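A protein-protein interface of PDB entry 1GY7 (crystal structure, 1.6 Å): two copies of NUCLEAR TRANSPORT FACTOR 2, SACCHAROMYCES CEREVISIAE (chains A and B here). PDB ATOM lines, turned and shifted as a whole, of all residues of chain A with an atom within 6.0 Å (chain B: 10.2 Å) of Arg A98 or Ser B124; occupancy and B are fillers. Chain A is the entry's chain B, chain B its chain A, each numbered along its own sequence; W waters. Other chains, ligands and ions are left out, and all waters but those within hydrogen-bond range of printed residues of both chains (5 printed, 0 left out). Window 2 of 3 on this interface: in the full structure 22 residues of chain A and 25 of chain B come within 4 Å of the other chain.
ND2 of Asn A122 lies close to NH2 of Arg B98 (2.7 Å). ND2 of Asn B122 is in hydrogen-bond range of OD1 of Asn A122, at 3.4 Å. The side-chain hydroxyl (OG) of Ser B100 is in hydrogen-bond range of the side-chain hydroxyl (OG) of Ser A100, 2.9 Å away.
Printed residues of chain B that touch a printed residue of chain A: Thr B68, Met B83, Arg B98, Ser B100, Asn B122, Tyr B123 and Ser B124. Hydrophobic or aromatic side chains of chain B that line the printed part of chain A: Met B83. Of the 15 printed residues of chain A, 5 touch a printed residue of chain B. Printed residues of chain A that touch a printed residue of chain B: Thr A85, Arg A98, Ser A100, Arg A120 and Asn A122. Along chain A the printed residues that touch a printed residue of chain B span positions 85 to 122. Among the printed residues, 13 pairs touch across the chains. Among the printed residues, no Asp or Glu carboxylate lies within 4 Å of a Lys or Arg side-chain nitrogen of the other chain.
Of the printed residues of chain B, Thr A85 touches Ser B100 (3.996 Å) and Asn B122 (3.3 Å). No residue of chain B comes within 4 Å of Gly A86. Leu A88 touches none of the printed residues of chain B. No residue of chain B comes within 4 Å of Gln A97. Printed residues of chain B within 4 Å of Ser A100: Met B83 (3.7 Å) and Ser B100 (2.9 Å). No residue of chain B comes within 4 Å of Leu A121. Asn A122 touches just these residues of chain B: Arg B98 (2.7 Å), Ser B100 (3.6 Å) and Asn B122 (3.4 Å). Of the printed residues of chain A, Ser B100 touches Thr A85 (3.996 Å), Ser A100 (2.9 Å) and Asn A122 (3.6 Å). Leu B121 touches none of the printed residues of chain A. Of the printed residues of chain A, Asn B122 touches Thr A85, Arg A98 and Asn A122. Of the printed residues of chain A, Ser B124 touches Arg A98.
The backbone carbonyl oxygen (O) of Arg B98 lies within hydrogen-bond range of the backbone NH (N) of Asn B122 (2.7 Å). ND2 of Asn B122 lies close to O of Phe B99 (3.5 Å). The guanidinium group of Arg B98 sits at hydrogen-bond distance from the side-chain hydroxyl of Thr B85 (3.5 Å). N of Ser A100 is in hydrogen-bond range of O of Arg A120 (2.9 Å). O of Arg A98 is in hydrogen-bond range of N of Asn A122, 2.8 Å away. The backbone NH (N) of Ser B100 is in hydrogen-bond range of the backbone carbonyl oxygen (O) of Arg B120 (2.8 Å).
Water W1 lies within hydrogen-bond range of OD1 of Asn A122 (2.6 Å), ND2 of Asn B122 (2.7 Å), O of Phe B99 (2.9 Å) and NE of Arg B98 (3.0 Å). Water W5 lies within hydrogen-bond range of O of Tyr A123 (2.7 Å) and NE of Arg B98 (3.1 Å). Water W3 bridges OG1 of Thr A85 (2.8 Å) and OD1 of Asn B122 (2.9 Å). Water W2 lies within hydrogen-bond range of the backbone carbonyl oxygen of Leu A121 (2.8 Å), the side-chain hydroxyl of Thr B85 (2.8 Å), the side-chain amide nitrogen of Asn A122 (3.2 Å) and the guanidinium group of Arg B98 (3.2 Å). Water W4 lies within hydrogen-bond range of the guanidinium group (NH1) of Arg A98 and the backbone carbonyl oxygen (O) of Asn B122.
Among the printed residues, merely in contact across the chains: Thr A85 with Ser B100 (3.996 Å), Thr A85 with Asn B122 (3.3 Å), Arg A98 with Arg B98 (3.7 Å), Arg A98 with Asn B122 (3.6 Å), Arg A98 with Tyr B123 (3.5 Å), Arg A98 with Ser B124 (3.7 Å), Ser A100 with Met B83 (3.7 Å), Arg A120 with Thr B68 (3.7 Å), Arg A120 with Met B83 (3.5 Å) and Asn A122 with Ser B100 (3.6 Å).
Thr A85 touches Ser B100, but with the chains exchanged Ser A100 does not touch Thr B85 (4.1 Å). Arg B98 touches its own counterpart, Arg A98. Arg A98 touches Asn B122, and with the chains exchanged Asn A122 touches Arg B98. Asn A122 touches Ser B100, but with the chains exchanged Ser A100 does not touch Asn B122 (4.6 Å). Of the 13 pairs that touch across the chains among the printed residues, 5 have their exchanged pair printed and touching as well.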
ATOM      1  N   THR A  85      15.731  10.944   2.487  1.00  0.00           N
ATOM      2  CA  THR A  85      14.329  11.353   2.551  1.00  0.00           C
ATOM      3  C   THR A  85      13.587  10.030   2.425  1.00  0.00           C
ATOM      4  O   THR A  85      13.978   9.158   1.643  1.00  0.00           O
ATOM      5  CB  THR A  85      13.891  12.313   1.408  1.00  0.00           C
ATOM      6  OG1 THR A  85      13.996  11.657   0.138  1.00  0.00           O
ATOM      7  CG2 THR A  85      14.743  13.569   1.417  1.00  0.00           C
ATOM      8  N   GLY A  86      12.539   9.857   3.217  1.00  0.00           N
ATOM      9  CA  GLY A  86      11.809   8.605   3.150  1.00  0.00           C
ATOM     10  C   GLY A  86      10.515   8.643   3.922  1.00  0.00           C
ATOM     11  O   GLY A  86      10.020   9.719   4.266  1.00  0.00           O
ATOM     12  N   ASP A  87       9.979   7.455   4.191  1.00  0.00           N
ATOM     13  CA  ASP A  87       8.729   7.296   4.919  1.00  0.00           C
ATOM     14  C   ASP A  87       8.929   6.458   6.164  1.00  0.00           C
ATOM     15  O   ASP A  87       9.771   5.561   6.204  1.00  0.00           O
ATOM     16  CB  ASP A  87       7.682   6.593   4.046  1.00  0.00           C
ATOM     17  CG  ASP A  87       7.176   7.465   2.926  1.00  0.00           C
ATOM     18  OD1 ASP A  87       6.559   6.920   1.987  1.00  0.00           O
ATOM     19  OD2 ASP A  87       7.386   8.693   2.989  1.00  0.00           O
ATOM     20  N   LEU A  88       8.130   6.751   7.177  1.00  0.00           N
ATOM     21  CA  LEU A  88       8.167   6.013   8.423  1.00  0.00           C
ATOM     22  C   LEU A  88       6.798   5.346   8.510  1.00  0.00           C
ATOM     23  O   LEU A  88       5.776   6.025   8.436  1.00  0.00           O
ATOM     24  CB  LEU A  88       8.358   6.980   9.593  1.00  0.00           C
ATOM     25  CG  LEU A  88       9.304   6.591  10.729  1.00  0.00           C
ATOM     26  CD1 LEU A  88      10.659   6.181  10.165  1.00  0.00           C
ATOM     27  CD2 LEU A  88       9.458   7.772  11.674  1.00  0.00           C
ATOM     28  N   PRO A  96       1.922   6.487   5.616  1.00  0.00           N
ATOM     29  CA  PRO A  96       3.303   6.960   5.745  1.00  0.00           C
ATOM     30  C   PRO A  96       3.523   8.333   6.362  1.00  0.00           C
ATOM     31  O   PRO A  96       2.795   9.286   6.086  1.00  0.00           O
ATOM     32  CB  PRO A  96       3.820   6.891   4.311  1.00  0.00           C
ATOM     33  CG  PRO A  96       2.601   7.220   3.515  1.00  0.00           C
ATOM     34  CD  PRO A  96       1.543   6.381   4.196  1.00  0.00           C
ATOM     35  N   GLN A  97       4.548   8.407   7.202  1.00  0.00           N
ATOM     36  CA  GLN A  97       4.956   9.636   7.868  1.00  0.00           C
ATOM     37  C   GLN A  97       6.304   9.960   7.227  1.00  0.00           C
ATOM     38  O   GLN A  97       7.307   9.312   7.530  1.00  0.00           O
ATOM     39  CB  GLN A  97       5.136   9.382   9.368  1.00  0.00           C
ATOM     40  CG  GLN A  97       5.665  10.562  10.169  1.00  0.00           C
ATOM     41  CD  GLN A  97       4.603  11.601  10.463  1.00  0.00           C
ATOM     42  OE1 GLN A  97       4.117  12.286   9.563  1.00  0.00           O
ATOM     43  NE2 GLN A  97       4.233  11.720  11.733  1.00  0.00           N
ATOM     44  N   ARG A  98       6.326  10.947   6.336  1.00  0.00           N
ATOM     45  CA  ARG A  98       7.565  11.304   5.651  1.00  0.00           C
ATOM     46  C   ARG A  98       8.559  12.022   6.547  1.00  0.00           C
ATOM     47  O   ARG A  98       8.175  12.733   7.473  1.00  0.00           O
ATOM     48  CB  ARG A  98       7.274  12.158   4.420  1.00  0.00           C
ATOM     49  CG  ARG A  98       8.489  12.327   3.529  1.00  0.00           C
ATOM     50  CD  ARG A  98       8.129  12.928   2.187  1.00  0.00           C
ATOM     51  NE  ARG A  98       7.532  14.252   2.324  1.00  0.00           N
ATOM     52  CZ  ARG A  98       7.223  15.033   1.296  1.00  0.00           C
ATOM     53  NH1 ARG A  98       7.456  14.618   0.056  1.00  0.00           N
ATOM     54  NH2 ARG A  98       6.682  16.226   1.504  1.00  0.00           N
ATOM     55  N   PHE A  99       9.844  11.835   6.256  1.00  0.00           N
ATOM     56  CA  PHE A  99      10.898  12.444   7.055  1.00  0.00           C
ATOM     57  C   PHE A  99      12.119  12.748   6.204  1.00  0.00           C
ATOM     58  O   PHE A  99      12.263  12.246   5.089  1.00  0.00           O
ATOM     59  CB  PHE A  99      11.324  11.486   8.173  1.00  0.00           C
ATOM     60  CG  PHE A  99      12.158  10.323   7.687  1.00  0.00           C
ATOM     61  CD1 PHE A  99      13.546  10.431   7.597  1.00  0.00           C
ATOM     62  CD2 PHE A  99      11.553   9.138   7.274  1.00  0.00           C
ATOM     63  CE1 PHE A  99      14.318   9.378   7.102  1.00  0.00           C
ATOM     64  CE2 PHE A  99      12.314   8.078   6.776  1.00  0.00           C
ATOM     65  CZ  PHE A  99      13.703   8.198   6.690  1.00  0.00           C
ATOM     66  N   SER A 100      12.990  13.587   6.752  1.00  0.00           N
ATOM     67  CA  SER A 100      14.248  13.931   6.113  1.00  0.00           C
ATOM     68  C   SER A 100      15.273  13.761   7.221  1.00  0.00           C
ATOM     69  O   SER A 100      15.017  14.123   8.369  1.00  0.00           O
ATOM     70  CB  SER A 100      14.236  15.374   5.607  1.00  0.00           C
ATOM     71  OG  SER A 100      13.451  15.480   4.431  1.00  0.00           O
ATOM     72  N   PHE A 119      17.115  15.044  12.389  1.00  0.00           N
ATOM     73  CA  PHE A 119      15.885  14.418  11.921  1.00  0.00           C
ATOM     74  C   PHE A 119      14.681  15.340  11.950  1.00  0.00           C
ATOM     75  O   PHE A 119      14.424  16.031  12.944  1.00  0.00           O
ATOM     76  CB  PHE A 119      15.591  13.188  12.783  1.00  0.00           C
ATOM     77  CG  PHE A 119      14.337  12.450  12.397  1.00  0.00           C
ATOM     78  CD1 PHE A 119      14.386  11.399  11.486  1.00  0.00           C
ATOM     79  CD2 PHE A 119      13.112  12.797  12.956  1.00  0.00           C
ATOM     80  CE1 PHE A 119      13.227  10.696  11.139  1.00  0.00           C
ATOM     81  CE2 PHE A 119      11.944  12.101  12.616  1.00  0.00           C
ATOM     82  CZ  PHE A 119      12.006  11.048  11.707  1.00  0.00           C
ATOM     83  N   ARG A 120      13.935  15.331  10.855  1.00  0.00           N
ATOM     84  CA  ARG A 120      12.736  16.141  10.750  1.00  0.00           C
ATOM     85  C   ARG A 120      11.610  15.373  10.099  1.00  0.00           C
ATOM     86  O   ARG A 120      11.838  14.556   9.209  1.00  0.00           O
ATOM     87  CB  ARG A 120      12.994  17.393   9.908  1.00  0.00           C
ATOM     88  CG  ARG A 120      13.688  18.519  10.643  1.00  0.00           C
ATOM     89  CD  ARG A 120      12.767  19.164  11.666  1.00  0.00           C
ATOM     90  NE  ARG A 120      13.361  20.389  12.192  1.00  0.00           N
ATOM     91  CZ  ARG A 120      12.763  21.208  13.049  1.00  0.00           C
ATOM     92  NH1 ARG A 120      11.540  20.937  13.491  1.00  0.00           N
ATOM     93  NH2 ARG A 120      13.393  22.301  13.458  1.00  0.00           N
ATOM     94  N   LEU A 121      10.395  15.623  10.570  1.00  0.00           N
ATOM     95  CA  LEU A 121       9.222  15.034   9.961  1.00  0.00           C
ATOM     96  C   LEU A 121       9.065  15.972   8.768  1.00  0.00           C
ATOM     97  O   LEU A 121       9.423  17.151   8.852  1.00  0.00           O
ATOM     98  CB  LEU A 121       8.018  15.141  10.900  1.00  0.00           C
ATOM     99  CG  LEU A 121       8.168  14.338  12.196  1.00  0.00           C
ATOM    100  CD1 LEU A 121       6.945  14.558  13.080  1.00  0.00           C
ATOM    101  CD2 LEU A 121       8.344  12.859  11.873  1.00  0.00           C
ATOM    102  N   ASN A 122       8.550  15.463   7.658  1.00  0.00           N
ATOM    103  CA  ASN A 122       8.401  16.277   6.460  1.00  0.00           C
ATOM    104  C   ASN A 122       7.019  16.005   5.880  1.00  0.00           C
ATOM    105  O   ASN A 122       6.858  15.163   4.999  1.00  0.00           O
ATOM    106  CB  ASN A 122       9.511  15.894   5.469  1.00  0.00           C
ATOM    107  CG  ASN A 122       9.732  16.936   4.392  1.00  0.00           C
ATOM    108  OD1 ASN A 122      10.697  16.854   3.629  1.00  0.00           O
ATOM    109  ND2 ASN A 122       8.844  17.917   4.318  1.00  0.00           N
ATOM    110  N   TYR A 123       6.024  16.721   6.399  1.00  0.00           N
ATOM    111  CA  TYR A 123       4.635  16.554   5.976  1.00  0.00           C
ATOM    112  C   TYR A 123       4.445  16.373   4.472  1.00  0.00           C
ATOM    113  O   TYR A 123       4.988  17.132   3.667  1.00  0.00           O
ATOM    114  CB  TYR A 123       3.792  17.740   6.452  1.00  0.00           C
ATOM    115  CG  TYR A 123       2.340  17.652   6.039  1.00  0.00           C
ATOM    116  CD1 TYR A 123       1.515  16.639   6.528  1.00  0.00           C
ATOM    117  CD2 TYR A 123       1.796  18.567   5.138  1.00  0.00           C
ATOM    118  CE1 TYR A 123       0.185  16.536   6.125  1.00  0.00           C
ATOM    119  CE2 TYR A 123       0.471  18.472   4.728  1.00  0.00           C
ATOM    120  CZ  TYR A 123      -0.329  17.455   5.225  1.00  0.00           C
ATOM    121  OH  TYR A 123      -1.638  17.352   4.817  1.00  0.00           O
ATOM    122  N   SER A 124       3.664  15.362   4.104  1.00  0.00           N
ATOM    123  CA  SER A 124       3.387  15.069   2.702  1.00  0.00           C
ATOM    124  C   SER A 124       2.084  15.735   2.274  1.00  0.00           C
ATOM    125  O   SER A 124       2.148  16.716   1.503  1.00  0.00           O
ATOM    126  CB  SER A 124       3.278  13.557   2.485  1.00  0.00           C
ATOM    127  OG  SER A 124       4.475  12.896   2.853  1.00  0.00           O
ATOM    128  OXT SER A 124       1.015  15.270   2.727  1.00  0.00           O
ATOM    129  N   THR B  67      10.865  26.054   5.914  1.00  0.00           N
ATOM    130  CA  THR B  67       9.880  25.611   6.895  1.00  0.00           C
ATOM    131  C   THR B  67      10.597  25.013   8.107  1.00  0.00           C
ATOM    132  O   THR B  67      10.049  24.994   9.207  1.00  0.00           O
ATOM    133  CB  THR B  67       8.850  24.615   6.296  1.00  0.00           C
ATOM    134  OG1 THR B  67       9.519  23.508   5.691  1.00  0.00           O
ATOM    135  CG2 THR B  67       7.995  25.317   5.254  1.00  0.00           C
ATOM    136  N   THR B  68      11.817  24.516   7.909  1.00  0.00           N
ATOM    137  CA  THR B  68      12.619  24.012   9.025  1.00  0.00           C
ATOM    138  C   THR B  68      14.099  24.265   8.768  1.00  0.00           C
ATOM    139  O   THR B  68      14.570  24.220   7.624  1.00  0.00           O
ATOM    140  CB  THR B  68      12.459  22.482   9.312  1.00  0.00           C
ATOM    141  OG1 THR B  68      13.083  21.717   8.268  1.00  0.00           O
ATOM    142  CG2 THR B  68      10.992  22.092   9.447  1.00  0.00           C
ATOM    143  N   MET B  83      20.724  21.555   8.068  1.00  0.00           N
ATOM    144  CA  MET B  83      19.736  20.848   7.262  1.00  0.00           C
ATOM    145  C   MET B  83      18.531  21.755   7.123  1.00  0.00           C
ATOM    146  O   MET B  83      18.064  22.340   8.098  1.00  0.00           O
ATOM    147  CB  MET B  83      19.299  19.522   7.894  1.00  0.00           C
ATOM    148  CG  MET B  83      18.324  18.759   7.003  1.00  0.00           C
ATOM    149  SD  MET B  83      17.834  17.110   7.588  1.00  0.00           S
ATOM    150  CE  MET B  83      16.402  17.521   8.595  1.00  0.00           C
ATOM    151  N   THR B  85      14.547  22.251   5.146  1.00  0.00           N
ATOM    152  CA  THR B  85      13.445  21.683   4.378  1.00  0.00           C
ATOM    153  C   THR B  85      12.556  22.889   4.147  1.00  0.00           C
ATOM    154  O   THR B  85      12.534  23.820   4.956  1.00  0.00           O
ATOM    155  CB  THR B  85      12.627  20.566   5.096  1.00  0.00           C
ATOM    156  OG1 THR B  85      11.920  21.106   6.218  1.00  0.00           O
ATOM    157  CG2 THR B  85      13.537  19.425   5.531  1.00  0.00           C
ATOM    158  N   GLY B  86      11.852  22.898   3.027  1.00  0.00           N
ATOM    159  CA  GLY B  86      10.998  24.030   2.750  1.00  0.00           C
ATOM    160  C   GLY B  86      10.246  23.878   1.454  1.00  0.00           C
ATOM    161  O   GLY B  86      10.179  22.791   0.877  1.00  0.00           O
ATOM    162  N   ASP B  87       9.675  24.990   1.011  1.00  0.00           N
ATOM    163  CA  ASP B  87       8.904  25.047  -0.218  1.00  0.00           C
ATOM    164  C   ASP B  87       9.673  25.843  -1.254  1.00  0.00           C
ATOM    165  O   ASP B  87      10.344  26.825  -0.933  1.00  0.00           O
ATOM    166  CB  ASP B  87       7.564  25.742   0.038  1.00  0.00           C
ATOM    167  CG  ASP B  87       6.676  24.973   0.997  1.00  0.00           C
ATOM    168  OD1 ASP B  87       5.733  25.582   1.544  1.00  0.00           O
ATOM    169  OD2 ASP B  87       6.908  23.760   1.192  1.00  0.00           O
ATOM    170  N   PRO B  96       3.679  25.013  -4.445  1.00  0.00           N
ATOM    171  CA  PRO B  96       5.127  24.884  -4.287  1.00  0.00           C
ATOM    172  C   PRO B  96       5.604  23.440  -4.314  1.00  0.00           C
ATOM    173  O   PRO B  96       4.818  22.503  -4.181  1.00  0.00           O
ATOM    174  CB  PRO B  96       5.377  25.539  -2.936  1.00  0.00           C
ATOM    175  CG  PRO B  96       4.169  25.133  -2.166  1.00  0.00           C
ATOM    176  CD  PRO B  96       3.046  25.384  -3.166  1.00  0.00           C
ATOM    177  N   GLN B  97       6.907  23.275  -4.493  1.00  0.00           N
ATOM    178  CA  GLN B  97       7.517  21.960  -4.508  1.00  0.00           C
ATOM    179  C   GLN B  97       8.316  21.845  -3.218  1.00  0.00           C
ATOM    180  O   GLN B  97       8.975  22.797  -2.807  1.00  0.00           O
ATOM    181  CB  GLN B  97       8.443  21.819  -5.717  1.00  0.00           C
ATOM    182  CG  GLN B  97       7.717  21.795  -7.058  1.00  0.00           C
ATOM    183  CD  GLN B  97       6.628  20.735  -7.105  1.00  0.00           C
ATOM    184  OE1 GLN B  97       6.845  19.590  -6.705  1.00  0.00           O
ATOM    185  NE2 GLN B  97       5.452  21.111  -7.600  1.00  0.00           N
ATOM    186  N   ARG B  98       8.243  20.691  -2.565  1.00  0.00           N
ATOM    187  CA  ARG B  98       8.983  20.488  -1.323  1.00  0.00           C
ATOM    188  C   ARG B  98      10.438  20.152  -1.616  1.00  0.00           C
ATOM    189  O   ARG B  98      10.735  19.407  -2.548  1.00  0.00           O
ATOM    190  CB  ARG B  98       8.361  19.346  -0.513  1.00  0.00           C
ATOM    191  CG  ARG B  98       7.019  19.682   0.104  1.00  0.00           C
ATOM    192  CD  ARG B  98       7.160  20.759   1.169  1.00  0.00           C
ATOM    193  NE  ARG B  98       7.982  20.313   2.292  1.00  0.00           N
ATOM    194  CZ  ARG B  98       8.339  21.088   3.311  1.00  0.00           C
ATOM    195  NH1 ARG B  98       7.949  22.355   3.348  1.00  0.00           N
ATOM    196  NH2 ARG B  98       9.079  20.595   4.297  1.00  0.00           N
ATOM    197  N   PHE B  99      11.346  20.704  -0.819  1.00  0.00           N
ATOM    198  CA  PHE B  99      12.763  20.420  -1.000  1.00  0.00           C
ATOM    199  C   PHE B  99      13.439  20.152   0.336  1.00  0.00           C
ATOM    200  O   PHE B  99      12.937  20.536   1.388  1.00  0.00           O
ATOM    201  CB  PHE B  99      13.467  21.588  -1.714  1.00  0.00           C
ATOM    202  CG  PHE B  99      13.813  22.753  -0.818  1.00  0.00           C
ATOM    203  CD1 PHE B  99      15.011  22.775  -0.107  1.00  0.00           C
ATOM    204  CD2 PHE B  99      12.944  23.834  -0.692  1.00  0.00           C
ATOM    205  CE1 PHE B  99      15.342  23.857   0.718  1.00  0.00           C
ATOM    206  CE2 PHE B  99      13.263  24.918   0.129  1.00  0.00           C
ATOM    207  CZ  PHE B  99      14.464  24.931   0.836  1.00  0.00           C
ATOM    208  N   SER B 100      14.574  19.464   0.275  1.00  0.00           N
ATOM    209  CA  SER B 100      15.382  19.169   1.452  1.00  0.00           C
ATOM    210  C   SER B 100      16.799  19.500   1.009  1.00  0.00           C
ATOM    211  O   SER B 100      17.186  19.202  -0.121  1.00  0.00           O
ATOM    212  CB  SER B 100      15.282  17.690   1.845  1.00  0.00           C
ATOM    213  OG  SER B 100      13.989  17.380   2.353  1.00  0.00           O
ATOM    214  N   ARG B 120      17.643  18.058  -2.815  1.00  0.00           N
ATOM    215  CA  ARG B 120      16.652  17.140  -3.365  1.00  0.00           C
ATOM    216  C   ARG B 120      15.251  17.713  -3.306  1.00  0.00           C
ATOM    217  O   ARG B 120      14.877  18.343  -2.322  1.00  0.00           O
ATOM    218  CB  ARG B 120      16.647  15.819  -2.586  1.00  0.00           C
ATOM    219  CG  ARG B 120      17.684  14.816  -3.018  1.00  0.00           C
ATOM    220  CD  ARG B 120      17.330  14.214  -4.374  1.00  0.00           C
ATOM    221  NE  ARG B 120      18.265  13.161  -4.746  1.00  0.00           N
ATOM    222  CZ  ARG B 120      18.167  12.428  -5.848  1.00  0.00           C
ATOM    223  NH1 ARG B 120      17.171  12.631  -6.699  1.00  0.00           N
ATOM    224  NH2 ARG B 120      19.062  11.483  -6.094  1.00  0.00           N
ATOM    225  N   LEU B 121      14.485  17.519  -4.375  1.00  0.00           N
ATOM    226  CA  LEU B 121      13.093  17.942  -4.363  1.00  0.00           C
ATOM    227  C   LEU B 121      12.415  16.666  -3.874  1.00  0.00           C
ATOM    228  O   LEU B 121      12.761  15.572  -4.327  1.00  0.00           O
ATOM    229  CB  LEU B 121      12.595  18.305  -5.762  1.00  0.00           C
ATOM    230  CG  LEU B 121      12.958  19.686  -6.311  1.00  0.00           C
ATOM    231  CD1 LEU B 121      12.223  19.920  -7.627  1.00  0.00           C
ATOM    232  CD2 LEU B 121      12.563  20.762  -5.306  1.00  0.00           C
ATOM    233  N   ASN B 122      11.481  16.797  -2.937  1.00  0.00           N
ATOM    234  CA  ASN B 122      10.794  15.638  -2.371  1.00  0.00           C
ATOM    235  C   ASN B 122       9.368  15.529  -2.886  1.00  0.00           C
ATOM    236  O   ASN B 122       8.606  16.493  -2.824  1.00  0.00           O
ATOM    237  CB  ASN B 122      10.780  15.743  -0.846  1.00  0.00           C
ATOM    238  CG  ASN B 122      12.094  16.258  -0.289  1.00  0.00           C
ATOM    239  OD1 ASN B 122      13.158  15.707  -0.566  1.00  0.00           O
ATOM    240  ND2 ASN B 122      12.024  17.323   0.503  1.00  0.00           N
ATOM    241  N   TYR B 123       9.002  14.353  -3.383  1.00  0.00           N
ATOM    242  CA  TYR B 123       7.659  14.149  -3.914  1.00  0.00           C
ATOM    243  C   TYR B 123       6.807  13.206  -3.078  1.00  0.00           C
ATOM    244  O   TYR B 123       7.283  12.176  -2.599  1.00  0.00           O
ATOM    245  CB  TYR B 123       7.727  13.626  -5.350  1.00  0.00           C
ATOM    246  CG  TYR B 123       8.474  14.541  -6.288  1.00  0.00           C
ATOM    247  CD1 TYR B 123       9.856  14.433  -6.446  1.00  0.00           C
ATOM    248  CD2 TYR B 123       7.800  15.528  -7.012  1.00  0.00           C
ATOM    249  CE1 TYR B 123      10.550  15.286  -7.294  1.00  0.00           C
ATOM    250  CE2 TYR B 123       8.483  16.389  -7.860  1.00  0.00           C
ATOM    251  CZ  TYR B 123       9.854  16.259  -8.000  1.00  0.00           C
ATOM    252  OH  TYR B 123      10.533  17.102  -8.840  1.00  0.00           O
ATOM    253  N   SER B 124       5.538  13.572  -2.920  1.00  0.00           N
ATOM    254  CA  SER B 124       4.584  12.780  -2.152  1.00  0.00           C
ATOM    255  C   SER B 124       4.184  11.528  -2.925  1.00  0.00           C
ATOM    256  O   SER B 124       4.208  10.430  -2.326  1.00  0.00           O
ATOM    257  CB  SER B 124       3.339  13.614  -1.842  1.00  0.00           C
ATOM    258  OG  SER B 124       2.737  14.096  -3.033  1.00  0.00           O
ATOM    259  OXT SER B 124       3.843  11.664  -4.118  1.00  0.00           O
HETATM  260  O   HOH W   1      10.633  18.943   2.102  1.00  0.00           O
HETATM  261  O   HOH W   2      10.014  19.146   6.981  1.00  0.00           O
HETATM  262  O   HOH W   3      12.496  13.103  -1.670  1.00  0.00           O
HETATM  263  O   HOH W   4       5.888  16.633  -1.229  1.00  0.00           O
HETATM  264  O   HOH W   5       5.412  19.831   3.959  1.00  0.00           O
